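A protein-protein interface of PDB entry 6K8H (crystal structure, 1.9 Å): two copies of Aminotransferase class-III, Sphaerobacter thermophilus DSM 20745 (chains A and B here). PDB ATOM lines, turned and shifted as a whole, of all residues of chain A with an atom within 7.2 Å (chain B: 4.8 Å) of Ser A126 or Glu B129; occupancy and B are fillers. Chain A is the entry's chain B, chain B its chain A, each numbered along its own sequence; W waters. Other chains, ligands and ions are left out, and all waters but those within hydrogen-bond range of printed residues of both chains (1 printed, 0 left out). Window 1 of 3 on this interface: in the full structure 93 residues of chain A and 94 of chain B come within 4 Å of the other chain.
The side-chain carboxylate (OE2) of Glu A129 lies within hydrogen-bond range of the side-chain hydroxyl (OG) of Ser B126 (2.5 Å). The side-chain hydroxyl (OG) of Ser A126 is in hydrogen-bond range of the side-chain carboxylate (OE2) of Glu B129, 2.5 Å away.
The backbone NH (N) of Glu B129 lies within hydrogen-bond range of the side-chain hydroxyl (OG) of Ser B126, 3.1 Å away. The side-chain hydroxyl of Thr A124 sits at hydrogen-bond distance from the backbone carbonyl oxygen of Ser A126. The backbone NH (N) of Asn A125 is in hydrogen-bond range of the side-chain carboxylate (OE1) of Glu A129. ND2 of Asn A125 lies within hydrogen-bond range of OD1 of Asn A319 (2.9 Å). The side-chain hydroxyl of Ser A126 lies within hydrogen-bond range of the backbone NH of Glu A129 (2.9 Å). The backbone NH of Ser A157 sits at hydrogen-bond distance from the side-chain hydroxyl of Thr A128.
Among the printed residues, merely in contact across the chains: Asn A125 with Asn B125 (3.5 Å), Thr A128 with Glu B129 (3.7 Å), Glu A129 with Thr B128 (3.8 Å) and Ser A157 with Met B132 (3.4 Å).
Of the printed residues of chain B, Ser A126 touches Glu B129. Of the printed residues of chain B, Glu A129 touches Ser B126 and Thr B128. Lys A282 touches none of the printed residues of chain B. Ala A292 touches none of the printed residues of chain B. Of the printed residues of chain A, Ser B126 touches Glu A129 (2.5 Å). Of the printed residues of chain A, Thr B128 touches Glu A129 (3.8 Å). Glu B129 touches just these residues of chain A: Ser A126 (2.5 Å) and Thr A128 (3.7 Å). The nearest printed residue of chain A that does not touch Thr B128 is Met A132 (4.1 Å).
Of the 20 printed residues of chain A, 5 touch a printed residue of chain B. Printed residues of chain A that touch a printed residue of chain B: Asn A125, Ser A126, Thr A128, Glu A129 and Ser A157. Of the 11 printed residues of chain B, 5 touch a printed residue of chain A. Hydrophobic or aromatic side chains of chain B that line the printed part of chain A: Met B132. Among the printed residues, 6 pairs touch across the chains. Among the printed residues, no Asp or Glu carboxylate lies within 4 Å of a Lys or Arg side-chain nitrogen of the other chain.
Asn B125 touches its own counterpart, Asn A125. Ser A126 touches Glu B129, and with the chains exchanged Glu A129 touches Ser B126. Thr A128 touches Glu B129, and with the chains exchanged Glu A129 touches Thr B128. Positions printed for both chains: 124, 125, 126, 127, 128, 129, 130, 131, 132 and 319. Of the 6 pairs that touch across the chains among the printed residues, 5 have their exchanged pair printed and touching as well.
Water W1 lies within hydrogen-bond range of the side-chain sulfur (SD) of Met B132 (3.0 Å) and the side-chain sulfur (SD) of Met A132 (3.1 Å).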
ATOM      1  N   PHE A 123      11.139  17.209  -7.642  1.00  0.00           N
ATOM      2  CA  PHE A 123      10.174  16.873  -8.679  1.00  0.00           C
ATOM      3  C   PHE A 123       8.749  16.950  -8.139  1.00  0.00           C
ATOM      4  O   PHE A 123       8.488  16.650  -6.965  1.00  0.00           O
ATOM      5  CB  PHE A 123      10.451  15.479  -9.244  1.00  0.00           C
ATOM      6  CG  PHE A 123      11.804  15.360  -9.873  1.00  0.00           C
ATOM      7  CD1 PHE A 123      12.016  15.821 -11.162  1.00  0.00           C
ATOM      8  CD2 PHE A 123      12.872  14.844  -9.161  1.00  0.00           C
ATOM      9  CE1 PHE A 123      13.266  15.746 -11.743  1.00  0.00           C
ATOM     10  CE2 PHE A 123      14.133  14.766  -9.737  1.00  0.00           C
ATOM     11  CZ  PHE A 123      14.330  15.222 -11.025  1.00  0.00           C
ATOM     12  N   THR A 124       7.837  17.385  -9.008  1.00  0.00           N
ATOM     13  CA  THR A 124       6.412  17.468  -8.730  1.00  0.00           C
ATOM     14  C   THR A 124       5.676  16.699  -9.822  1.00  0.00           C
ATOM     15  O   THR A 124       6.316  16.063 -10.667  1.00  0.00           O
ATOM     16  CB  THR A 124       5.952  18.923  -8.697  1.00  0.00           C
ATOM     17  OG1 THR A 124       6.070  19.465 -10.016  1.00  0.00           O
ATOM     18  CG2 THR A 124       6.811  19.757  -7.725  1.00  0.00           C
ATOM     19  N   ASN A 125       4.346  16.772  -9.840  1.00  0.00           N
ATOM     20  CA  ASN A 125       3.562  16.015 -10.806  1.00  0.00           C
ATOM     21  C   ASN A 125       2.980  16.873 -11.923  1.00  0.00           C
ATOM     22  O   ASN A 125       2.227  16.349 -12.759  1.00  0.00           O
ATOM     23  CB  ASN A 125       2.464  15.245 -10.077  1.00  0.00           C
ATOM     24  CG  ASN A 125       3.038  14.370  -8.998  1.00  0.00           C
ATOM     25  OD1 ASN A 125       3.685  13.368  -9.299  1.00  0.00           O
ATOM     26  ND2 ASN A 125       2.886  14.779  -7.743  1.00  0.00           N
ATOM     27  N   SER A 126       3.307  18.166 -11.964  1.00  0.00           N
ATOM     28  CA  SER A 126       2.805  19.055 -13.007  1.00  0.00           C
ATOM     29  C   SER A 126       3.634  20.330 -12.976  1.00  0.00           C
ATOM     30  O   SER A 126       4.272  20.652 -11.965  1.00  0.00           O
ATOM     31  CB  SER A 126       1.323  19.364 -12.843  1.00  0.00           C
ATOM     32  OG  SER A 126       1.116  20.037 -11.632  1.00  0.00           O
ATOM     33  N   GLY A 127       3.624  21.045 -14.104  1.00  0.00           N
ATOM     34  CA  GLY A 127       4.193  22.382 -14.117  1.00  0.00           C
ATOM     35  C   GLY A 127       3.451  23.327 -13.192  1.00  0.00           C
ATOM     36  O   GLY A 127       4.048  24.209 -12.573  1.00  0.00           O
ATOM     37  N   THR A 128       2.127  23.160 -13.101  1.00  0.00           N
ATOM     38  CA  THR A 128       1.338  23.901 -12.122  1.00  0.00           C
ATOM     39  C   THR A 128       1.875  23.693 -10.714  1.00  0.00           C
ATOM     40  O   THR A 128       2.032  24.656  -9.947  1.00  0.00           O
ATOM     41  CB  THR A 128      -0.118  23.461 -12.189  1.00  0.00           C
ATOM     42  OG1 THR A 128      -0.683  23.946 -13.398  1.00  0.00           O
ATOM     43  CG2 THR A 128      -0.907  24.014 -10.971  1.00  0.00           C
ATOM     44  N   GLU A 129       2.135  22.434 -10.346  1.00  0.00           N
ATOM     45  CA  GLU A 129       2.678  22.147  -9.023  1.00  0.00           C
ATOM     46  C   GLU A 129       4.068  22.740  -8.867  1.00  0.00           C
ATOM     47  O   GLU A 129       4.419  23.241  -7.796  1.00  0.00           O
ATOM     48  CB  GLU A 129       2.716  20.632  -8.763  1.00  0.00           C
ATOM     49  CG  GLU A 129       1.376  20.009  -8.359  1.00  0.00           C
ATOM     50  CD  GLU A 129       1.512  18.576  -7.788  1.00  0.00           C
ATOM     51  OE1 GLU A 129       2.619  17.986  -7.827  1.00  0.00           O
ATOM     52  OE2 GLU A 129       0.493  18.041  -7.300  1.00  0.00           O
ATOM     53  N   ALA A 130       4.884  22.676  -9.919  1.00  0.00           N
ATOM     54  CA  ALA A 130       6.224  23.251  -9.844  1.00  0.00           C
ATOM     55  C   ALA A 130       6.162  24.746  -9.560  1.00  0.00           C
ATOM     56  O   ALA A 130       6.868  25.254  -8.680  1.00  0.00           O
ATOM     57  CB  ALA A 130       6.974  22.977 -11.149  1.00  0.00           C
ATOM     58  N   VAL A 131       5.299  25.462 -10.284  1.00  0.00           N
ATOM     59  CA  VAL A 131       5.143  26.903 -10.074  1.00  0.00           C
ATOM     60  C   VAL A 131       4.639  27.180  -8.663  1.00  0.00           C
ATOM     61  O   VAL A 131       5.124  28.092  -7.976  1.00  0.00           O
ATOM     62  CB  VAL A 131       4.199  27.496 -11.139  1.00  0.00           C
ATOM     63  CG1 VAL A 131       3.864  28.957 -10.832  1.00  0.00           C
ATOM     64  CG2 VAL A 131       4.835  27.367 -12.543  1.00  0.00           C
ATOM     65  N   MET A 132       3.648  26.406  -8.213  1.00  0.00           N
ATOM     66  CA  MET A 132       3.132  26.595  -6.863  1.00  0.00           C
ATOM     67  C   MET A 132       4.236  26.408  -5.829  1.00  0.00           C
ATOM     68  O   MET A 132       4.394  27.226  -4.921  1.00  0.00           O
ATOM     69  CB  MET A 132       1.986  25.620  -6.594  1.00  0.00           C
ATOM     70  CG  MET A 132       1.520  25.646  -5.148  1.00  0.00           C
ATOM     71  SD  MET A 132       0.072  24.591  -4.884  1.00  0.00           S
ATOM     72  CE  MET A 132       0.826  22.987  -4.586  1.00  0.00           C
ATOM     73  N   SER A 157      -2.743  26.514 -13.123  1.00  0.00           N
ATOM     74  CA  SER A 157      -4.027  26.713 -12.451  1.00  0.00           C
ATOM     75  C   SER A 157      -3.910  27.099 -10.969  1.00  0.00           C
ATOM     76  O   SER A 157      -4.936  27.197 -10.283  1.00  0.00           O
ATOM     77  CB  SER A 157      -4.906  25.458 -12.622  1.00  0.00           C
ATOM     78  OG  SER A 157      -4.230  24.291 -12.226  1.00  0.00           O
ATOM     79  N   VAL A 257       8.657  26.045 -17.909  1.00  0.00           N
ATOM     80  CA  VAL A 257       7.917  24.810 -18.168  1.00  0.00           C
ATOM     81  C   VAL A 257       7.861  24.533 -19.669  1.00  0.00           C
ATOM     82  O   VAL A 257       7.982  23.380 -20.102  1.00  0.00           O
ATOM     83  CB  VAL A 257       6.515  24.879 -17.531  1.00  0.00           C
ATOM     84  CG1 VAL A 257       5.657  23.697 -17.978  1.00  0.00           C
ATOM     85  CG2 VAL A 257       6.633  24.879 -16.006  1.00  0.00           C
ATOM     86  N   MET A 280       9.894  23.946 -13.998  1.00  0.00           N
ATOM     87  CA  MET A 280      10.058  23.158 -15.212  1.00  0.00           C
ATOM     88  C   MET A 280       8.979  22.091 -15.244  1.00  0.00           C
ATOM     89  O   MET A 280       8.340  21.791 -14.232  1.00  0.00           O
ATOM     90  CB  MET A 280      11.445  22.489 -15.266  1.00  0.00           C
ATOM     91  CG  MET A 280      12.611  23.452 -15.128  1.00  0.00           C
ATOM     92  SD  MET A 280      14.137  22.638 -14.596  1.00  0.00           S
ATOM     93  CE  MET A 280      13.964  22.736 -12.805  1.00  0.00           C
ATOM     94  N   GLY A 281       8.816  21.486 -16.410  1.00  0.00           N
ATOM     95  CA  GLY A 281       7.867  20.406 -16.611  1.00  0.00           C
ATOM     96  C   GLY A 281       7.919  19.967 -18.056  1.00  0.00           C
ATOM     97  O   GLY A 281       8.961  20.117 -18.699  1.00  0.00           O
ATOM     98  N   LYS A 282       6.809  19.426 -18.571  1.00  0.00           N
ATOM     99  CA  LYS A 282       6.670  19.047 -19.978  1.00  0.00           C
ATOM    100  C   LYS A 282       7.804  18.132 -20.466  1.00  0.00           C
ATOM    101  O   LYS A 282       7.788  16.923 -20.167  1.00  0.00           O
ATOM    102  CB  LYS A 282       6.530  20.323 -20.823  1.00  0.00           C
ATOM    103  CG  LYS A 282       5.217  21.085 -20.511  1.00  0.00           C
ATOM    104  CD  LYS A 282       4.884  22.185 -21.521  1.00  0.00           C
ATOM    105  CE  LYS A 282       3.377  22.562 -21.513  1.00  0.00           C
ATOM    106  NZ  LYS A 282       2.990  23.544 -20.441  1.00  0.00           N
ATOM    107  N   PRO A 289       3.501  12.518 -16.663  1.00  0.00           N
ATOM    108  CA  PRO A 289       3.222  13.692 -15.821  1.00  0.00           C
ATOM    109  C   PRO A 289       4.431  14.050 -14.965  1.00  0.00           C
ATOM    110  O   PRO A 289       5.077  13.182 -14.377  1.00  0.00           O
ATOM    111  CB  PRO A 289       2.022  13.248 -14.974  1.00  0.00           C
ATOM    112  CG  PRO A 289       1.390  12.127 -15.748  1.00  0.00           C
ATOM    113  CD  PRO A 289       2.539  11.425 -16.409  1.00  0.00           C
ATOM    114  N   VAL A 290       4.741  15.341 -14.909  1.00  0.00           N
ATOM    115  CA  VAL A 290       6.003  15.776 -14.316  1.00  0.00           C
ATOM    116  C   VAL A 290       6.007  17.278 -14.086  1.00  0.00           C
ATOM    117  O   VAL A 290       5.356  18.042 -14.814  1.00  0.00           O
ATOM    118  CB  VAL A 290       7.185  15.389 -15.221  1.00  0.00           C
ATOM    119  CG1 VAL A 290       7.132  16.201 -16.500  1.00  0.00           C
ATOM    120  CG2 VAL A 290       8.530  15.553 -14.497  1.00  0.00           C
ATOM    121  N   GLY A 291       6.751  17.702 -13.071  1.00  0.00           N
ATOM    122  CA  GLY A 291       7.201  19.073 -12.935  1.00  0.00           C
ATOM    123  C   GLY A 291       8.454  19.054 -12.086  1.00  0.00           C
ATOM    124  O   GLY A 291       8.845  18.022 -11.539  1.00  0.00           O
ATOM    125  N   ALA A 292       9.076  20.214 -11.961  1.00  0.00           N
ATOM    126  CA  ALA A 292      10.265  20.285 -11.122  1.00  0.00           C
ATOM    127  C   ALA A 292      10.500  21.729 -10.749  1.00  0.00           C
ATOM    128  O   ALA A 292      10.243  22.628 -11.543  1.00  0.00           O
ATOM    129  CB  ALA A 292      11.511  19.717 -11.828  1.00  0.00           C
ATOM    130  N   ASN A 319       5.442  12.035  -6.661  1.00  0.00           N
ATOM    131  CA  ASN A 319       6.671  12.825  -6.912  1.00  0.00           C
ATOM    132  C   ASN A 319       7.816  11.849  -7.192  1.00  0.00           C
ATOM    133  O   ASN A 319       7.998  10.913  -6.415  1.00  0.00           O
ATOM    134  CB  ASN A 319       7.110  13.634  -5.686  1.00  0.00           C
ATOM    135  CG  ASN A 319       6.149  14.729  -5.274  1.00  0.00           C
ATOM    136  OD1 ASN A 319       5.097  14.889  -5.866  1.00  0.00           O
ATOM    137  ND2 ASN A 319       6.523  15.495  -4.265  1.00  0.00           N
ATOM    138  N   THR B 124      -7.120  15.266 -13.040  1.00  0.00           N
ATOM    139  CA  THR B 124      -5.991  16.122 -12.725  1.00  0.00           C
ATOM    140  C   THR B 124      -4.756  15.240 -12.626  1.00  0.00           C
ATOM    141  O   THR B 124      -4.828  14.028 -12.869  1.00  0.00           O
ATOM    142  CB  THR B 124      -6.211  16.880 -11.407  1.00  0.00           C
ATOM    143  OG1 THR B 124      -6.244  15.950 -10.314  1.00  0.00           O
ATOM    144  CG2 THR B 124      -7.526  17.672 -11.419  1.00  0.00           C
ATOM    145  N   ASN B 125      -3.639  15.816 -12.212  1.00  0.00           N
ATOM    146  CA  ASN B 125      -2.389  15.083 -12.160  1.00  0.00           C
ATOM    147  C   ASN B 125      -1.972  14.683 -10.745  1.00  0.00           C
ATOM    148  O   ASN B 125      -0.869  14.144 -10.571  1.00  0.00           O
ATOM    149  CB  ASN B 125      -1.306  15.917 -12.835  1.00  0.00           C
ATOM    150  CG  ASN B 125      -1.642  16.185 -14.273  1.00  0.00           C
ATOM    151  OD1 ASN B 125      -1.635  15.268 -15.096  1.00  0.00           O
ATOM    152  ND2 ASN B 125      -2.001  17.432 -14.580  1.00  0.00           N
ATOM    153  N   SER B 126      -2.810  14.938  -9.743  1.00  0.00           N
ATOM    154  CA  SER B 126      -2.458  14.624  -8.361  1.00  0.00           C
ATOM    155  C   SER B 126      -3.700  14.821  -7.502  1.00  0.00           C
ATOM    156  O   SER B 126      -4.617  15.554  -7.878  1.00  0.00           O
ATOM    157  CB  SER B 126      -1.291  15.451  -7.851  1.00  0.00           C
ATOM    158  OG  SER B 126      -1.618  16.825  -7.872  1.00  0.00           O
ATOM    159  N   GLY B 127      -3.708  14.192  -6.322  1.00  0.00           N
ATOM    160  CA  GLY B 127      -4.770  14.485  -5.364  1.00  0.00           C
ATOM    161  C   GLY B 127      -4.729  15.920  -4.888  1.00  0.00           C
ATOM    162  O   GLY B 127      -5.772  16.534  -4.648  1.00  0.00           O
ATOM    163  N   THR B 128      -3.520  16.467  -4.733  1.00  0.00           N
ATOM    164  CA  THR B 128      -3.372  17.880  -4.399  1.00  0.00           C
ATOM    165  C   THR B 128      -4.110  18.751  -5.404  1.00  0.00           C
ATOM    166  O   THR B 128      -4.882  19.645  -5.024  1.00  0.00           O
ATOM    167  CB  THR B 128      -1.888  18.272  -4.344  1.00  0.00           C
ATOM    168  OG1 THR B 128      -1.316  17.802  -3.118  1.00  0.00           O
ATOM    169  CG2 THR B 128      -1.730  19.792  -4.418  1.00  0.00           C
ATOM    170  N   GLU B 129      -3.905  18.481  -6.702  1.00  0.00           N
ATOM    171  CA  GLU B 129      -4.602  19.236  -7.739  1.00  0.00           C
ATOM    172  C   GLU B 129      -6.111  19.002  -7.694  1.00  0.00           C
ATOM    173  O   GLU B 129      -6.896  19.932  -7.912  1.00  0.00           O
ATOM    174  CB  GLU B 129      -4.052  18.875  -9.124  1.00  0.00           C
ATOM    175  CG  GLU B 129      -2.757  19.597  -9.484  1.00  0.00           C
ATOM    176  CD  GLU B 129      -2.374  19.439 -10.943  1.00  0.00           C
ATOM    177  OE1 GLU B 129      -3.083  18.735 -11.712  1.00  0.00           O
ATOM    178  OE2 GLU B 129      -1.350  20.048 -11.318  1.00  0.00           O
ATOM    179  N   ALA B 130      -6.539  17.761  -7.451  1.00  0.00           N
ATOM    180  CA  ALA B 130      -7.972  17.494  -7.352  1.00  0.00           C
ATOM    181  C   ALA B 130      -8.608  18.313  -6.228  1.00  0.00           C
ATOM    182  O   ALA B 130      -9.695  18.876  -6.402  1.00  0.00           O
ATOM    183  CB  ALA B 130      -8.220  16.005  -7.118  1.00  0.00           C
ATOM    184  N   VAL B 131      -7.956  18.366  -5.062  1.00  0.00           N
ATOM    185  CA  VAL B 131      -8.484  19.137  -3.933  1.00  0.00           C
ATOM    186  C   VAL B 131      -8.538  20.624  -4.275  1.00  0.00           C
ATOM    187  O   VAL B 131      -9.540  21.312  -4.007  1.00  0.00           O
ATOM    188  CB  VAL B 131      -7.643  18.871  -2.666  1.00  0.00           C
ATOM    189  CG1 VAL B 131      -8.063  19.803  -1.525  1.00  0.00           C
ATOM    190  CG2 VAL B 131      -7.810  17.431  -2.233  1.00  0.00           C
ATOM    191  N   MET B 132      -7.462  21.141  -4.883  1.00  0.00           N
ATOM    192  CA  MET B 132      -7.453  22.536  -5.300  1.00  0.00           C
ATOM    193  C   MET B 132      -8.596  22.824  -6.270  1.00  0.00           C
ATOM    194  O   MET B 132      -9.294  23.835  -6.148  1.00  0.00           O
ATOM    195  CB  MET B 132      -6.109  22.878  -5.941  1.00  0.00           C
ATOM    196  CG  MET B 132      -6.082  24.229  -6.648  1.00  0.00           C
ATOM    197  SD  MET B 132      -4.422  24.638  -7.254  1.00  0.00           S
ATOM    198  CE  MET B 132      -4.430  23.793  -8.839  1.00  0.00           C
ATOM    199  N   MET B 133      -8.794  21.952  -7.255  1.00  0.00           N
ATOM    200  CA  MET B 133      -9.799  22.249  -8.262  1.00  0.00           C
ATOM    201  C   MET B 133     -11.214  22.088  -7.713  1.00  0.00           C
ATOM    202  O   MET B 133     -12.125  22.774  -8.180  1.00  0.00           O
ATOM    203  CB  MET B 133      -9.582  21.376  -9.492  1.00  0.00           C
ATOM    204  CG  MET B 133      -8.277  21.676 -10.268  1.00  0.00           C
ATOM    205  SD  MET B 133      -7.972  23.432 -10.583  1.00  0.00           S
ATOM    206  CE  MET B 133      -9.447  23.852 -11.524  1.00  0.00           C
ATOM    207  N   ASN B 319      -3.382  16.149 -17.896  1.00  0.00           N
ATOM    208  CA  ASN B 319      -4.753  15.757 -17.569  1.00  0.00           C
ATOM    209  C   ASN B 319      -5.210  14.638 -18.485  1.00  0.00           C
ATOM    210  O   ASN B 319      -5.156  14.763 -19.713  1.00  0.00           O
ATOM    211  CB  ASN B 319      -5.720  16.936 -17.722  1.00  0.00           C
ATOM    212  CG  ASN B 319      -5.504  18.030 -16.699  1.00  0.00           C
ATOM    213  OD1 ASN B 319      -4.512  18.041 -15.978  1.00  0.00           O
ATOM    214  ND2 ASN B 319      -6.440  18.979 -16.652  1.00  0.00           N
HETATM  215  O   HOH W   1      -1.804  23.158  -6.925  1.00  0.00           O
